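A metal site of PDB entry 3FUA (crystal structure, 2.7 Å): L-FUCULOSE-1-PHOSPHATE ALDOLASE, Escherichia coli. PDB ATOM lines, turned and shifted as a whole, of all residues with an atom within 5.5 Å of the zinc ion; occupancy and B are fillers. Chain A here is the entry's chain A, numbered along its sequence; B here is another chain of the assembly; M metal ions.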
ATOM      1  N   ALA A  27     -25.489  14.436   2.588  1.00  0.00           N
ATOM      2  CA  ALA A  27     -24.780  15.595   3.110  1.00  0.00           C
ATOM      3  C   ALA A  27     -23.254  15.494   2.960  1.00  0.00           C
ATOM      4  O   ALA A  27     -22.672  14.397   2.974  1.00  0.00           O
ATOM      5  CB  ALA A  27     -25.208  15.868   4.556  1.00  0.00           C
ATOM      6  N   ASN A  29     -19.169  17.304   3.739  1.00  0.00           N
ATOM      7  CA  ASN A  29     -18.298  17.596   4.853  1.00  0.00           C
ATOM      8  C   ASN A  29     -17.225  18.551   4.334  1.00  0.00           C
ATOM      9  O   ASN A  29     -16.841  18.490   3.166  1.00  0.00           O
ATOM     10  CB  ASN A  29     -17.679  16.325   5.465  1.00  0.00           C
ATOM     11  CG  ASN A  29     -17.711  15.125   4.528  1.00  0.00           C
ATOM     12  OD1 ASN A  29     -16.764  14.876   3.782  1.00  0.00           O
ATOM     13  ND2 ASN A  29     -18.782  14.353   4.595  1.00  0.00           N
ATOM     14  N   GLU A  73     -16.144  10.533   6.869  1.00  0.00           N
ATOM     15  CA  GLU A  73     -15.370  10.572   5.635  1.00  0.00           C
ATOM     16  C   GLU A  73     -14.111  11.416   5.798  1.00  0.00           C
ATOM     17  O   GLU A  73     -13.567  11.924   4.827  1.00  0.00           O
ATOM     18  CB  GLU A  73     -16.225  11.126   4.502  1.00  0.00           C
ATOM     19  CG  GLU A  73     -17.540  10.371   4.332  1.00  0.00           C
ATOM     20  CD  GLU A  73     -18.264  10.777   3.065  1.00  0.00           C
ATOM     21  OE1 GLU A  73     -19.005  11.790   3.092  1.00  0.00           O
ATOM     22  OE2 GLU A  73     -18.072  10.085   2.050  1.00  0.00           O
ATOM     23  N   PHE A  76     -10.284  10.750   3.606  1.00  0.00           N
ATOM     24  CA  PHE A  76      -9.880  11.298   2.322  1.00  0.00           C
ATOM     25  C   PHE A  76      -9.640  12.794   2.246  1.00  0.00           C
ATOM     26  O   PHE A  76      -9.174  13.305   1.234  1.00  0.00           O
ATOM     27  CB  PHE A  76     -10.667  10.710   1.135  1.00  0.00           C
ATOM     28  CG  PHE A  76     -12.142  10.978   1.141  1.00  0.00           C
ATOM     29  CD1 PHE A  76     -12.646  12.237   1.410  1.00  0.00           C
ATOM     30  CD2 PHE A  76     -13.022   9.964   0.763  1.00  0.00           C
ATOM     31  CE1 PHE A  76     -14.029  12.482   1.287  1.00  0.00           C
ATOM     32  CE2 PHE A  76     -14.395  10.203   0.633  1.00  0.00           C
ATOM     33  CZ  PHE A  76     -14.888  11.455   0.896  1.00  0.00           C
ATOM     34  N   HIS A  92     -16.390  18.343   0.252  1.00  0.00           N
ATOM     35  CA  HIS A  92     -16.879  17.101  -0.315  1.00  0.00           C
ATOM     36  C   HIS A  92     -18.389  17.044  -0.236  1.00  0.00           C
ATOM     37  O   HIS A  92     -18.971  17.376   0.797  1.00  0.00           O
ATOM     38  CB  HIS A  92     -16.316  15.899   0.431  1.00  0.00           C
ATOM     39  CG  HIS A  92     -17.033  14.616   0.114  1.00  0.00           C
ATOM     40  ND1 HIS A  92     -17.061  14.019  -1.125  1.00  0.00           N
ATOM     41  CD2 HIS A  92     -17.785  13.811   0.920  1.00  0.00           C
ATOM     42  CE1 HIS A  92     -17.798  12.901  -1.051  1.00  0.00           C
ATOM     43  NE2 HIS A  92     -18.262  12.734   0.177  1.00  0.00           N
ATOM     44  N   ASN A  93     -19.045  16.645  -1.319  1.00  0.00           N
ATOM     45  CA  ASN A  93     -20.497  16.531  -1.288  1.00  0.00           C
ATOM     46  C   ASN A  93     -20.948  15.392  -2.188  1.00  0.00           C
ATOM     47  O   ASN A  93     -20.126  14.665  -2.734  1.00  0.00           O
ATOM     48  CB  ASN A  93     -21.175  17.837  -1.682  1.00  0.00           C
ATOM     49  CG  ASN A  93     -21.005  18.165  -3.150  1.00  0.00           C
ATOM     50  OD1 ASN A  93     -21.124  17.288  -4.013  1.00  0.00           O
ATOM     51  ND2 ASN A  93     -20.722  19.425  -3.442  1.00  0.00           N
ATOM     52  N   HIS A  94     -22.267  15.207  -2.265  1.00  0.00           N
ATOM     53  CA  HIS A  94     -22.870  14.183  -3.113  1.00  0.00           C
ATOM     54  C   HIS A  94     -23.893  14.886  -4.010  1.00  0.00           C
ATOM     55  O   HIS A  94     -25.017  14.434  -4.172  1.00  0.00           O
ATOM     56  CB  HIS A  94     -23.582  13.144  -2.253  1.00  0.00           C
ATOM     57  CG  HIS A  94     -22.699  12.456  -1.251  1.00  0.00           C
ATOM     58  ND1 HIS A  94     -22.935  11.197  -0.765  1.00  0.00           N
ATOM     59  CD2 HIS A  94     -21.577  12.879  -0.630  1.00  0.00           C
ATOM     60  CE1 HIS A  94     -21.968  10.902   0.120  1.00  0.00           C
ATOM     61  NE2 HIS A  94     -21.116  11.892   0.233  1.00  0.00           N
ATOM     62  N   HIS A 155     -20.447   7.712  -5.967  1.00  0.00           N
ATOM     63  CA  HIS A 155     -20.319   8.442  -4.699  1.00  0.00           C
ATOM     64  C   HIS A 155     -20.615   9.942  -4.729  1.00  0.00           C
ATOM     65  O   HIS A 155     -21.627  10.373  -4.198  1.00  0.00           O
ATOM     66  CB  HIS A 155     -18.941   8.153  -4.075  1.00  0.00           C
ATOM     67  CG  HIS A 155     -18.787   8.644  -2.668  1.00  0.00           C
ATOM     68  ND1 HIS A 155     -17.896   8.103  -1.773  1.00  0.00           N
ATOM     69  CD2 HIS A 155     -19.396   9.657  -2.000  1.00  0.00           C
ATOM     70  CE1 HIS A 155     -18.007   8.787  -0.617  1.00  0.00           C
ATOM     71  NE2 HIS A 155     -18.906   9.745  -0.711  1.00  0.00           N
ATOM     72  N   TYR B 113     -24.313   4.063  -3.026  1.00  0.00           N
ATOM     73  CA  TYR B 113     -24.236   3.384  -1.735  1.00  0.00           C
ATOM     74  C   TYR B 113     -25.257   3.776  -0.667  1.00  0.00           C
ATOM     75  O   TYR B 113     -25.489   3.007   0.270  1.00  0.00           O
ATOM     76  CB  TYR B 113     -22.808   3.498  -1.186  1.00  0.00           C
ATOM     77  CG  TYR B 113     -22.452   4.803  -0.490  1.00  0.00           C
ATOM     78  CD1 TYR B 113     -22.726   4.970   0.855  1.00  0.00           C
ATOM     79  CD2 TYR B 113     -21.804   5.815  -1.158  1.00  0.00           C
ATOM     80  CE1 TYR B 113     -22.348   6.115   1.523  1.00  0.00           C
ATOM     81  CE2 TYR B 113     -21.417   6.973  -0.488  1.00  0.00           C
ATOM     82  CZ  TYR B 113     -21.699   7.112   0.854  1.00  0.00           C
ATOM     83  OH  TYR B 113     -21.310   8.235   1.529  1.00  0.00           O
HETATM   84 ZN    ZN M   1     -19.309  11.079   0.684  1.00  0.00          ZN
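A ring nitrogen (NE2) of His 155 binds the zinc ion, 2.0 Å away.
The zinc ion is bound by a ring nitrogen (NE2) of His 92 (2.0 Å).
A ring nitrogen (NE2) of His 94 is bound to the zinc ion (2.0 Å).
The zinc ion is bound by OE2 of Glu 73 (2.1 Å).
OE1 of Glu 73 is bound to the zinc ion, at 2.5 Å.
The zinc ion has five donor atoms within binding distance.
Merely in contact with the zinc ion: Tyr 113 of chain B.
Five residues have an atom within 4 Å of the zinc ion: Glu 73, His 92, His 94, His 155 and Tyr 113 of chain B.
Along chain A the residues within 4 Å of the zinc ion span positions 73 to 155.
The nearest printed residue that does not touch the zinc ion is Phe 76 (4.4 Å).
The backbone carbonyl oxygen (O) of His 92 is in hydrogen-bond range of the backbone NH (N) of Asn 29, at 2.9 Å.
The side-chain amide nitrogen of Asn 29 sits close to the side-chain carboxylate of Glu 73 (3.0 Å).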
